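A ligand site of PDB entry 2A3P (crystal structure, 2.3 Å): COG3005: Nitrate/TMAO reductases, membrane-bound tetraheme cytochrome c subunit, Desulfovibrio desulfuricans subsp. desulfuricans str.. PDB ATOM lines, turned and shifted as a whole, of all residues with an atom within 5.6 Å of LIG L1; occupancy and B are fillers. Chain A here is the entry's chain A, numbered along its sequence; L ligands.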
ATOM      1  N   ALA A  24      -0.602  32.463   0.422  1.00  0.00           N
ATOM      2  CA  ALA A  24      -2.049  32.256   0.689  1.00  0.00           C
ATOM      3  C   ALA A  24      -2.260  31.871   2.153  1.00  0.00           C
ATOM      4  O   ALA A  24      -1.300  31.657   2.895  1.00  0.00           O
ATOM      5  CB  ALA A  24      -2.622  31.203  -0.239  1.00  0.00           C
ATOM      6  N   GLU A  25      -3.527  31.772   2.552  1.00  0.00           N
ATOM      7  CA  GLU A  25      -3.909  31.614   3.951  1.00  0.00           C
ATOM      8  C   GLU A  25      -4.359  30.201   4.228  1.00  0.00           C
ATOM      9  O   GLU A  25      -5.091  29.617   3.435  1.00  0.00           O
ATOM     10  CB  GLU A  25      -5.035  32.595   4.277  1.00  0.00           C
ATOM     11  CG  GLU A  25      -4.606  33.832   5.040  1.00  0.00           C
ATOM     12  CD  GLU A  25      -3.232  34.324   4.655  1.00  0.00           C
ATOM     13  OE1 GLU A  25      -2.370  34.400   5.554  1.00  0.00           O
ATOM     14  OE2 GLU A  25      -3.006  34.631   3.463  1.00  0.00           O
ATOM     15  N   ALA A  26      -3.924  29.645   5.347  1.00  0.00           N
ATOM     16  CA  ALA A  26      -4.383  28.320   5.739  1.00  0.00           C
ATOM     17  C   ALA A  26      -5.911  28.361   5.908  1.00  0.00           C
ATOM     18  O   ALA A  26      -6.455  29.374   6.352  1.00  0.00           O
ATOM     19  CB  ALA A  26      -3.704  27.902   7.026  1.00  0.00           C
ATOM     20  N   PRO A  27      -6.611  27.298   5.506  1.00  0.00           N
ATOM     21  CA  PRO A  27      -8.037  27.259   5.755  1.00  0.00           C
ATOM     22  C   PRO A  27      -8.346  26.896   7.204  1.00  0.00           C
ATOM     23  O   PRO A  27      -7.458  26.470   7.953  1.00  0.00           O
ATOM     24  CB  PRO A  27      -8.550  26.181   4.797  1.00  0.00           C
ATOM     25  CG  PRO A  27      -7.405  25.305   4.569  1.00  0.00           C
ATOM     26  CD  PRO A  27      -6.163  26.115   4.755  1.00  0.00           C
ATOM     27  N   LEU A  31     -11.283  20.220   8.391  1.00  0.00           N
ATOM     28  CA  LEU A  31     -11.328  19.813   6.990  1.00  0.00           C
ATOM     29  C   LEU A  31     -11.331  18.271   6.869  1.00  0.00           C
ATOM     30  O   LEU A  31     -10.489  17.603   7.458  1.00  0.00           O
ATOM     31  CB  LEU A  31     -10.123  20.401   6.269  1.00  0.00           C
ATOM     32  CG  LEU A  31     -10.012  20.464   4.739  1.00  0.00           C
ATOM     33  CD1 LEU A  31      -8.863  21.401   4.347  1.00  0.00           C
ATOM     34  CD2 LEU A  31      -9.802  19.071   4.113  1.00  0.00           C
ATOM     35  N   LYS A  32     -12.276  17.729   6.102  1.00  0.00           N
ATOM     36  CA  LYS A  32     -12.353  16.277   5.905  1.00  0.00           C
ATOM     37  C   LYS A  32     -11.593  15.793   4.678  1.00  0.00           C
ATOM     38  O   LYS A  32     -11.811  16.264   3.556  1.00  0.00           O
ATOM     39  CB  LYS A  32     -13.809  15.803   5.845  1.00  0.00           C
ATOM     40  CG  LYS A  32     -14.522  15.778   7.179  1.00  0.00           C
ATOM     41  N   MET A  33     -10.672  14.856   4.910  1.00  0.00           N
ATOM     42  CA  MET A  33     -10.033  14.097   3.864  1.00  0.00           C
ATOM     43  C   MET A  33     -10.832  12.813   3.687  1.00  0.00           C
ATOM     44  O   MET A  33     -10.768  11.901   4.533  1.00  0.00           O
ATOM     45  CB  MET A  33      -8.564  13.804   4.218  1.00  0.00           C
ATOM     46  CG  MET A  33      -7.687  15.068   4.235  1.00  0.00           C
ATOM     47  SD  MET A  33      -5.971  14.754   4.693  1.00  0.00           S
ATOM     48  CE  MET A  33      -5.296  14.132   3.148  1.00  0.00           C
ATOM     49  N   ASN A  35     -11.469  10.657   0.555  1.00  0.00           N
ATOM     50  CA  ASN A  35     -11.377   9.861  -0.667  1.00  0.00           C
ATOM     51  C   ASN A  35     -11.512   8.353  -0.383  1.00  0.00           C
ATOM     52  O   ASN A  35     -11.613   7.541  -1.309  1.00  0.00           O
ATOM     53  CB  ASN A  35     -10.059  10.139  -1.376  1.00  0.00           C
ATOM     54  CG  ASN A  35      -9.913  11.586  -1.760  1.00  0.00           C
ATOM     55  OD1 ASN A  35     -10.450  12.034  -2.777  1.00  0.00           O
ATOM     56  ND2 ASN A  35      -9.206  12.343  -0.947  1.00  0.00           N
ATOM     57  N   PHE A  42      -8.315  16.995   8.969  1.00  0.00           N
ATOM     58  CA  PHE A  42      -7.058  17.720   8.929  1.00  0.00           C
ATOM     59  C   PHE A  42      -7.207  19.156   9.425  1.00  0.00           C
ATOM     60  O   PHE A  42      -7.974  19.943   8.865  1.00  0.00           O
ATOM     61  CB  PHE A  42      -6.397  17.694   7.543  1.00  0.00           C
ATOM     62  CG  PHE A  42      -5.040  18.351   7.515  1.00  0.00           C
ATOM     63  CD1 PHE A  42      -3.903  17.624   7.905  1.00  0.00           C
ATOM     64  CD2 PHE A  42      -4.903  19.685   7.174  1.00  0.00           C
ATOM     65  CE1 PHE A  42      -2.639  18.232   7.896  1.00  0.00           C
ATOM     66  CE2 PHE A  42      -3.655  20.296   7.175  1.00  0.00           C
ATOM     67  CZ  PHE A  42      -2.516  19.557   7.532  1.00  0.00           C
ATOM     68  N   HIS A  44      -5.222  22.595   9.955  1.00  0.00           N
ATOM     69  CA  HIS A  44      -4.061  23.411   9.602  1.00  0.00           C
ATOM     70  C   HIS A  44      -3.400  24.012  10.847  1.00  0.00           C
ATOM     71  O   HIS A  44      -2.187  24.225  10.859  1.00  0.00           O
ATOM     72  CB  HIS A  44      -4.424  24.481   8.518  1.00  0.00           C
ATOM     73  CG  HIS A  44      -4.344  23.961   7.106  1.00  0.00           C
ATOM     74  ND1 HIS A  44      -5.384  23.287   6.499  1.00  0.00           N
ATOM     75  CD2 HIS A  44      -3.336  23.967   6.200  1.00  0.00           C
ATOM     76  CE1 HIS A  44      -5.031  22.929   5.279  1.00  0.00           C
ATOM     77  NE2 HIS A  44      -3.791  23.328   5.057  1.00  0.00           N
ATOM     78  N   HIS A  47      -0.454  22.345  12.336  1.00  0.00           N
ATOM     79  CA  HIS A  47       0.602  22.206  11.339  1.00  0.00           C
ATOM     80  C   HIS A  47       1.141  23.558  10.875  1.00  0.00           C
ATOM     81  O   HIS A  47       1.908  23.635   9.914  1.00  0.00           O
ATOM     82  CB  HIS A  47       0.088  21.376  10.159  1.00  0.00           C
ATOM     83  CG  HIS A  47      -0.243  19.954  10.521  1.00  0.00           C
ATOM     84  ND1 HIS A  47      -1.534  19.545  10.799  1.00  0.00           N
ATOM     85  CD2 HIS A  47       0.540  18.860  10.647  1.00  0.00           C
ATOM     86  CE1 HIS A  47      -1.519  18.248  11.088  1.00  0.00           C
ATOM     87  NE2 HIS A  47      -0.270  17.804  10.996  1.00  0.00           N
ATOM     88  N   TYR A  50       4.796  24.615  10.064  1.00  0.00           N
ATOM     89  CA  TYR A  50       5.379  24.105   8.823  1.00  0.00           C
ATOM     90  C   TYR A  50       5.097  25.016   7.649  1.00  0.00           C
ATOM     91  O   TYR A  50       4.055  25.658   7.588  1.00  0.00           O
ATOM     92  CB  TYR A  50       4.915  22.671   8.563  1.00  0.00           C
ATOM     93  CG  TYR A  50       5.377  21.721   9.677  1.00  0.00           C
ATOM     94  CD1 TYR A  50       4.498  21.288  10.684  1.00  0.00           C
ATOM     95  CD2 TYR A  50       6.722  21.314   9.757  1.00  0.00           C
ATOM     96  CE1 TYR A  50       4.928  20.438  11.708  1.00  0.00           C
ATOM     97  CE2 TYR A  50       7.159  20.469  10.793  1.00  0.00           C
ATOM     98  CZ  TYR A  50       6.254  20.040  11.752  1.00  0.00           C
ATOM     99  OH  TYR A  50       6.706  19.219  12.768  1.00  0.00           O
ATOM    100  N   GLN A  51       6.057  25.101   6.735  1.00  0.00           N
ATOM    101  CA  GLN A  51       5.869  25.886   5.521  1.00  0.00           C
ATOM    102  C   GLN A  51       4.773  25.260   4.683  1.00  0.00           C
ATOM    103  O   GLN A  51       4.650  24.029   4.617  1.00  0.00           O
ATOM    104  CB  GLN A  51       7.175  25.983   4.730  1.00  0.00           C
ATOM    105  CG  GLN A  51       8.151  27.083   5.229  1.00  0.00           C
ATOM    106  CD  GLN A  51       7.669  28.511   4.904  1.00  0.00           C
ATOM    107  OE1 GLN A  51       8.317  29.243   4.148  1.00  0.00           O
ATOM    108  NE2 GLN A  51       6.539  28.897   5.477  1.00  0.00           N
ATOM    109  N   CYS A  52       3.953  26.103   4.055  1.00  0.00           N
ATOM    110  CA  CYS A  52       2.910  25.630   3.139  1.00  0.00           C
ATOM    111  C   CYS A  52       3.443  24.545   2.202  1.00  0.00           C
ATOM    112  O   CYS A  52       2.846  23.455   2.083  1.00  0.00           O
ATOM    113  CB  CYS A  52       2.324  26.788   2.346  1.00  0.00           C
ATOM    114  SG  CYS A  52       1.509  28.020   3.376  1.00  0.00           S
ATOM    115  N   ASP A  54       5.797  22.461   2.363  1.00  0.00           N
ATOM    116  CA  ASP A  54       6.176  21.179   2.966  1.00  0.00           C
ATOM    117  C   ASP A  54       5.181  20.074   2.635  1.00  0.00           C
ATOM    118  O   ASP A  54       5.542  18.897   2.574  1.00  0.00           O
ATOM    119  CB  ASP A  54       6.360  21.305   4.493  1.00  0.00           C
ATOM    120  CG  ASP A  54       7.684  21.962   4.890  1.00  0.00           C
ATOM    121  OD1 ASP A  54       7.868  22.237   6.090  1.00  0.00           O
ATOM    122  OD2 ASP A  54       8.550  22.186   4.011  1.00  0.00           O
ATOM    123  N   CYS A  55       3.916  20.462   2.420  1.00  0.00           N
ATOM    124  CA  CYS A  55       2.881  19.521   1.988  1.00  0.00           C
ATOM    125  C   CYS A  55       2.322  19.910   0.614  1.00  0.00           C
ATOM    126  O   CYS A  55       2.138  19.055  -0.258  1.00  0.00           O
ATOM    127  CB  CYS A  55       1.767  19.458   3.013  1.00  0.00           C
ATOM    128  SG  CYS A  55       2.374  19.319   4.747  1.00  0.00           S
ATOM    129  N   HIS A  56       2.042  21.189   0.420  1.00  0.00           N
ATOM    130  CA  HIS A  56       1.602  21.676  -0.884  1.00  0.00           C
ATOM    131  C   HIS A  56       2.834  21.957  -1.761  1.00  0.00           C
ATOM    132  O   HIS A  56       3.112  23.106  -2.123  1.00  0.00           O
ATOM    133  CB  HIS A  56       0.726  22.921  -0.721  1.00  0.00           C
ATOM    134  CG  HIS A  56      -0.474  22.733   0.179  1.00  0.00           C
ATOM    135  ND1 HIS A  56      -1.645  22.128  -0.252  1.00  0.00           N
ATOM    136  CD2 HIS A  56      -0.692  23.090   1.469  1.00  0.00           C
ATOM    137  CE1 HIS A  56      -2.519  22.128   0.740  1.00  0.00           C
ATOM    138  NE2 HIS A  56      -1.974  22.707   1.795  1.00  0.00           N
ATOM    139  N   LEU A  65      -1.986  24.181  -4.735  1.00  0.00           N
ATOM    140  CA  LEU A  65      -2.861  24.019  -3.571  1.00  0.00           C
ATOM    141  C   LEU A  65      -3.997  23.051  -3.845  1.00  0.00           C
ATOM    142  O   LEU A  65      -4.963  22.983  -3.067  1.00  0.00           O
ATOM    143  CB  LEU A  65      -3.382  25.381  -3.083  1.00  0.00           C
ATOM    144  CG  LEU A  65      -2.302  26.362  -2.589  1.00  0.00           C
ATOM    145  CD1 LEU A  65      -2.847  27.785  -2.440  1.00  0.00           C
ATOM    146  CD2 LEU A  65      -1.637  25.895  -1.308  1.00  0.00           C
ATOM    147  N   ALA A  66      -3.885  22.321  -4.954  1.00  0.00           N
ATOM    148  CA  ALA A  66      -4.904  21.336  -5.344  1.00  0.00           C
ATOM    149  C   ALA A  66      -4.967  20.152  -4.387  1.00  0.00           C
ATOM    150  O   ALA A  66      -3.967  19.793  -3.730  1.00  0.00           O
ATOM    151  CB  ALA A  66      -4.679  20.861  -6.764  1.00  0.00           C
ATOM    152  N   LYS A  67      -6.144  19.536  -4.326  1.00  0.00           N
ATOM    153  CA  LYS A  67      -6.336  18.390  -3.459  1.00  0.00           C
ATOM    154  C   LYS A  67      -5.441  17.244  -3.923  1.00  0.00           C
ATOM    155  O   LYS A  67      -5.320  16.990  -5.111  1.00  0.00           O
ATOM    156  CB  LYS A  67      -7.810  18.006  -3.399  1.00  0.00           C
ATOM    157  CG  LYS A  67      -8.711  19.188  -2.999  1.00  0.00           C
ATOM    158  CD  LYS A  67      -9.053  19.196  -1.505  1.00  0.00           C
ATOM    159  CE  LYS A  67     -10.469  18.685  -1.245  1.00  0.00           C
ATOM    160  NZ  LYS A  67     -10.627  17.199  -1.447  1.00  0.00           N
ATOM    161  N   CYS A  68      -4.782  16.607  -2.956  1.00  0.00           N
ATOM    162  CA  CYS A  68      -3.785  15.562  -3.180  1.00  0.00           C
ATOM    163  C   CYS A  68      -4.210  14.477  -4.185  1.00  0.00           C
ATOM    164  O   CYS A  68      -3.438  14.119  -5.075  1.00  0.00           O
ATOM    165  CB  CYS A  68      -3.361  14.944  -1.840  1.00  0.00           C
ATOM    166  SG  CYS A  68      -2.932  16.200  -0.584  1.00  0.00           S
ATOM    167  N   ALA A  69      -5.441  13.996  -4.061  1.00  0.00           N
ATOM    168  CA  ALA A  69      -5.942  12.932  -4.943  1.00  0.00           C
ATOM    169  C   ALA A  69      -6.608  13.438  -6.238  1.00  0.00           C
ATOM    170  O   ALA A  69      -7.395  12.713  -6.858  1.00  0.00           O
ATOM    171  CB  ALA A  69      -6.871  11.991  -4.176  1.00  0.00           C
ATOM    172  N   TYR A  87      -1.932   7.375  -3.554  1.00  0.00           N
ATOM    173  CA  TYR A  87      -2.515   8.106  -2.427  1.00  0.00           C
ATOM    174  C   TYR A  87      -2.121   7.498  -1.081  1.00  0.00           C
ATOM    175  O   TYR A  87      -1.778   8.225  -0.157  1.00  0.00           O
ATOM    176  CB  TYR A  87      -4.046   8.133  -2.537  1.00  0.00           C
ATOM    177  CG  TYR A  87      -4.739   9.089  -1.569  1.00  0.00           C
ATOM    178  CD1 TYR A  87      -4.463  10.458  -1.587  1.00  0.00           C
ATOM    179  CD2 TYR A  87      -5.700   8.626  -0.674  1.00  0.00           C
ATOM    180  CE1 TYR A  87      -5.111  11.340  -0.718  1.00  0.00           C
ATOM    181  CE2 TYR A  87      -6.369   9.503   0.202  1.00  0.00           C
ATOM    182  CZ  TYR A  87      -6.058  10.852   0.168  1.00  0.00           C
ATOM    183  OH  TYR A  87      -6.690  11.744   1.023  1.00  0.00           O
HETATM  184 FE1  LIG L   1      -2.931  22.978   3.397  1.00  0.00          FE
HETATM  185  C1  LIG L   1      -5.839  21.613   2.242  1.00  0.00           C
HETATM  186  C2  LIG L   1      -3.746  25.998   2.146  1.00  0.00           C
HETATM  187  C3  LIG L   1      -0.252  24.441   5.149  1.00  0.00           C
HETATM  188  C4  LIG L   1      -1.722  19.898   4.276  1.00  0.00           C
HETATM  189  N1  LIG L   1      -4.524  23.670   2.405  1.00  0.00           N
HETATM  190  C5  LIG L   1      -5.593  22.944   1.945  1.00  0.00           C
HETATM  191  C6  LIG L   1      -6.405  23.806   1.125  1.00  0.00           C
HETATM  192  C7  LIG L   1      -5.831  25.024   1.103  1.00  0.00           C
HETATM  193  C8  LIG L   1      -4.623  24.957   1.917  1.00  0.00           C
HETATM  194  C9  LIG L   1      -6.310  26.293   0.356  1.00  0.00           C
HETATM  195  C10 LIG L   1      -7.704  23.368   0.402  1.00  0.00           C
HETATM  196  C11 LIG L   1      -8.907  23.575   1.308  1.00  0.00           C
HETATM  197  C12 LIG L   1     -10.189  23.207   0.590  1.00  0.00           C
HETATM  198  O1  LIG L   1     -11.244  23.765   0.973  1.00  0.00           O
HETATM  199  O2  LIG L   1     -10.150  22.365  -0.347  1.00  0.00           O
HETATM  200  N2  LIG L   1      -2.167  24.887   3.672  1.00  0.00           N
HETATM  201  C13 LIG L   1      -2.625  25.974   2.939  1.00  0.00           C
HETATM  202  C14 LIG L   1      -1.696  27.060   3.143  1.00  0.00           C
HETATM  203  C15 LIG L   1      -0.730  26.640   3.981  1.00  0.00           C
HETATM  204  C16 LIG L   1      -1.009  25.268   4.333  1.00  0.00           C
HETATM  205  C17 LIG L   1      -1.836  28.444   2.493  1.00  0.00           C
HETATM  206  C18 LIG L   1       0.484  27.459   4.495  1.00  0.00           C
HETATM  207  C19 LIG L   1       0.284  28.447   5.391  1.00  0.00           C
HETATM  208  N3  LIG L   1      -1.276  22.310   4.545  1.00  0.00           N
HETATM  209  C20 LIG L   1      -0.267  23.067   5.113  1.00  0.00           C
HETATM  210  C21 LIG L   1       0.737  22.165   5.632  1.00  0.00           C
HETATM  211  C22 LIG L   1       0.341  20.914   5.389  1.00  0.00           C
HETATM  212  C23 LIG L   1      -0.947  20.980   4.700  1.00  0.00           C
HETATM  213  C24 LIG L   1       2.042  22.587   6.332  1.00  0.00           C
HETATM  214  C25 LIG L   1       1.118  19.615   5.753  1.00  0.00           C
HETATM  215  C26 LIG L   1       1.149  19.207   7.037  1.00  0.00           C
HETATM  216  N4  LIG L   1      -3.689  21.032   3.285  1.00  0.00           N
HETATM  217  C27 LIG L   1      -3.006  19.912   3.730  1.00  0.00           C
HETATM  218  C28 LIG L   1      -3.854  18.754   3.508  1.00  0.00           C
HETATM  219  C29 LIG L   1      -5.129  19.298   2.863  1.00  0.00           C
HETATM  220  C30 LIG L   1      -4.938  20.717   2.765  1.00  0.00           C
HETATM  221  C31 LIG L   1      -3.581  17.268   3.816  1.00  0.00           C
HETATM  222  C32 LIG L   1      -6.358  18.483   2.421  1.00  0.00           C
HETATM  223  C33 LIG L   1      -6.212  18.191   0.928  1.00  0.00           C
HETATM  224  C34 LIG L   1      -7.183  17.154   0.437  1.00  0.00           C
HETATM  225  O3  LIG L   1      -6.825  16.462  -0.547  1.00  0.00           O
HETATM  226  O4  LIG L   1      -8.320  17.005   0.993  1.00  0.00           O
HETATM  227 FE1  LG2 L   2       0.270  16.047  11.447  1.00  0.00          FE
HETATM  228  C1  LG2 L   2      -0.709  16.577  14.723  1.00  0.00           C
HETATM  229  C2  LG2 L   2      -2.868  14.677  10.822  1.00  0.00           C
HETATM  230  C3  LG2 L   2       1.011  15.678   8.113  1.00  0.00           C
HETATM  231  C4  LG2 L   2       3.413  17.097  12.106  1.00  0.00           C
HETATM  232  N1  LG2 L   2      -1.487  15.747  12.556  1.00  0.00           N
HETATM  233  C5  LG2 L   2      -1.623  15.959  13.913  1.00  0.00           C
HETATM  234  C6  LG2 L   2      -2.884  15.385  14.335  1.00  0.00           C
HETATM  235  C7  LG2 L   2      -3.478  14.851  13.243  1.00  0.00           C
HETATM  236  C8  LG2 L   2      -2.617  15.086  12.112  1.00  0.00           C
HETATM  237  C9  LG2 L   2      -4.850  14.126  13.128  1.00  0.00           C
HETATM  238  C10 LG2 L   2      -3.405  15.407  15.800  1.00  0.00           C
HETATM  239  C11 LG2 L   2      -4.080  16.724  16.202  1.00  0.00           C
HETATM  240  C12 LG2 L   2      -5.196  17.069  15.235  1.00  0.00           C
HETATM  241  O1  LG2 L   2      -6.242  16.376  15.203  1.00  0.00           O
HETATM  242  O2  LG2 L   2      -5.034  18.055  14.469  1.00  0.00           O
HETATM  243  N2  LG2 L   2      -0.766  15.331   9.763  1.00  0.00           N
HETATM  244  C13 LG2 L   2      -2.007  14.751   9.764  1.00  0.00           C
HETATM  245  C14 LG2 L   2      -2.259  14.240   8.444  1.00  0.00           C
HETATM  246  C15 LG2 L   2      -1.188  14.512   7.677  1.00  0.00           C
HETATM  247  C16 LG2 L   2      -0.229  15.211   8.497  1.00  0.00           C
HETATM  248  C17 LG2 L   2      -3.574  13.515   8.067  1.00  0.00           C
HETATM  249  C18 LG2 L   2      -0.977  14.164   6.172  1.00  0.00           C
HETATM  250  C19 LG2 L   2      -1.675  14.819   5.233  1.00  0.00           C
HETATM  251  N3  LG2 L   2       1.893  16.347  10.329  1.00  0.00           N
HETATM  252  C20 LG2 L   2       2.006  16.102   8.965  1.00  0.00           C
HETATM  253  C21 LG2 L   2       3.382  16.374   8.595  1.00  0.00           C
HETATM  254  C22 LG2 L   2       4.039  16.764   9.702  1.00  0.00           C
HETATM  255  C23 LG2 L   2       3.111  16.758  10.805  1.00  0.00           C
HETATM  256  C24 LG2 L   2       3.908  16.208   7.147  1.00  0.00           C
HETATM  257  C25 LG2 L   2       5.536  17.161   9.837  1.00  0.00           C
HETATM  258  C26 LG2 L   2       6.108  17.895   8.871  1.00  0.00           C
HETATM  259  N4  LG2 L   2       1.211  16.747  13.155  1.00  0.00           N
HETATM  260  C27 LG2 L   2       2.556  17.093  13.187  1.00  0.00           C
HETATM  261  C28 LG2 L   2       2.912  17.465  14.529  1.00  0.00           C
HETATM  262  C29 LG2 L   2       1.625  17.292  15.356  1.00  0.00           C
HETATM  263  C30 LG2 L   2       0.619  16.847  14.413  1.00  0.00           C
HETATM  264  C31 LG2 L   2       4.308  17.907  15.035  1.00  0.00           C
HETATM  265  C32 LG2 L   2       1.405  17.560  16.871  1.00  0.00           C
HETATM  266  C33 LG2 L   2       0.930  19.011  16.989  1.00  0.00           C
HETATM  267  C34 LG2 L   2      -0.426  19.181  17.628  1.00  0.00           C
HETATM  268  O3  LG2 L   2      -0.985  20.320  17.505  1.00  0.00           O
HETATM  269  O4  LG2 L   2      -0.972  18.221  18.272  1.00  0.00           O
HETATM  270 FE1  LG3 L   3       2.339  15.372  -4.506  1.00  0.00          FE
HETATM  271  C1  LG3 L   3       5.378  13.907  -5.020  1.00  0.00           C
HETATM  272  C2  LG3 L   3       2.501  14.694  -1.154  1.00  0.00           C
HETATM  273  C3  LG3 L   3      -0.538  17.250  -3.969  1.00  0.00           C
HETATM  274  C4  LG3 L   3       1.810  15.616  -7.917  1.00  0.00           C
HETATM  275  N1  LG3 L   3       3.716  14.531  -3.292  1.00  0.00           N
HETATM  276  C5  LG3 L   3       4.857  13.868  -3.736  1.00  0.00           C
HETATM  277  C6  LG3 L   3       5.406  13.138  -2.606  1.00  0.00           C
HETATM  278  C7  LG3 L   3       4.613  13.354  -1.546  1.00  0.00           C
HETATM  279  C8  LG3 L   3       3.527  14.226  -1.956  1.00  0.00           C
HETATM  280  C9  LG3 L   3       4.782  12.766  -0.130  1.00  0.00           C
HETATM  281  C10 LG3 L   3       6.682  12.253  -2.667  1.00  0.00           C
HETATM  282  C11 LG3 L   3       6.268  10.877  -3.180  1.00  0.00           C
HETATM  283  C12 LG3 L   3       7.442   9.944  -3.440  1.00  0.00           C
HETATM  284  O1  LG3 L   3       7.407   9.180  -4.447  1.00  0.00           O
HETATM  285  O2  LG3 L   3       8.410   9.943  -2.635  1.00  0.00           O
HETATM  286  N2  LG3 L   3       1.190  15.925  -2.842  1.00  0.00           N
HETATM  287  C13 LG3 L   3       1.429  15.460  -1.566  1.00  0.00           C
HETATM  288  C14 LG3 L   3       0.341  15.917  -0.727  1.00  0.00           C
HETATM  289  C15 LG3 L   3      -0.524  16.633  -1.490  1.00  0.00           C
HETATM  290  C16 LG3 L   3      -0.002  16.639  -2.841  1.00  0.00           C
HETATM  291  C17 LG3 L   3       0.255  15.600   0.788  1.00  0.00           C
HETATM  292  C18 LG3 L   3      -1.836  17.314  -1.003  1.00  0.00           C
HETATM  293  C19 LG3 L   3      -1.804  18.299  -0.072  1.00  0.00           C
HETATM  294  N3  LG3 L   3       0.918  16.294  -5.740  1.00  0.00           N
HETATM  295  C20 LG3 L   3      -0.220  16.965  -5.293  1.00  0.00           C
HETATM  296  C21 LG3 L   3      -0.999  17.330  -6.475  1.00  0.00           C
HETATM  297  C22 LG3 L   3      -0.374  16.886  -7.565  1.00  0.00           C
HETATM  298  C23 LG3 L   3       0.856  16.227  -7.121  1.00  0.00           C
HETATM  299  C24 LG3 L   3      -2.343  18.100  -6.431  1.00  0.00           C
HETATM  300  C25 LG3 L   3      -0.904  17.036  -9.033  1.00  0.00           C
HETATM  301  C26 LG3 L   3      -0.632  18.115  -9.802  1.00  0.00           C
HETATM  302  N4  LG3 L   3       3.432  14.778  -6.250  1.00  0.00           N
HETATM  303  C27 LG3 L   3       3.055  15.121  -7.540  1.00  0.00           C
HETATM  304  C28 LG3 L   3       4.201  14.893  -8.417  1.00  0.00           C
HETATM  305  C29 LG3 L   3       5.324  14.365  -7.516  1.00  0.00           C
HETATM  306  C30 LG3 L   3       4.751  14.316  -6.176  1.00  0.00           C
HETATM  307  C31 LG3 L   3       4.316  15.127  -9.954  1.00  0.00           C
HETATM  308  C32 LG3 L   3       6.737  13.981  -8.027  1.00  0.00           C
HETATM  309  C33 LG3 L   3       7.895  14.361  -7.106  1.00  0.00           C
HETATM  310  C34 LG3 L   3       7.963  15.820  -6.727  1.00  0.00           C
HETATM  311  O3  LG3 L   3       7.517  16.706  -7.513  1.00  0.00           O
HETATM  312  O4  LG3 L   3       8.503  16.113  -5.628  1.00  0.00           O
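A carbon (C18) of LIG L1 is bonded to the side-chain sulfur (SG) of Cys 52, 1.6 Å away. The side-chain sulfur (SG) of Cys 55 is bonded to a carbon (C25) of LIG L1, at 1.6 Å. NE2 of His 56 binds FE1 of LIG L1, at 1.9 Å. An iron atom (FE1) of LIG L1 is bound by a ring nitrogen (NE2) of His 44 (1.9 Å). An oxygen (O3) of LIG L1 lies within hydrogen-bond range of the backbone NH (N) of Cys 68 (3.2 Å). The side-chain amino group of Lys 67 lies within salt-bridge range of an oxygen (O4) of LIG L1. A ring nitrogen (NE2) of His 47 is bound to an iron atom (FE1) of LG2 L2 (1.9 Å). A carbon (C18) of LG3 L3 is bonded to the side-chain sulfur (SG) of Cys 68, at 1.6 Å.
Merely in contact with LIG L1: Ala 24 (3.3 Å), Phe 42 (3.4 Å), Pro 27 (3.4 Å), Gln 51 (3.4 Å), Glu 25 (3.5 Å), Met 33 (3.6 Å), Tyr 50 (3.6 Å), His 47 (3.7 Å), Leu 31 (3.7 Å) and Ala 26 (3.7 Å). Hydrophobic or aromatic side chains within 4 Å of LIG L1: Ala 24, Pro 27, Leu 31, Met 33, Phe 42, His 44, His 47, Tyr 50 and His 56. Of the 23 residues printed, 16 come within 4 Å of LIG L1.
The backbone NH (N) of Phe 42 is in hydrogen-bond range of the backbone carbonyl oxygen (O) of Leu 31 (2.7 Å). N of Gln 51 lies within hydrogen-bond range of OD1 of Asp 54, 3.4 Å away.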
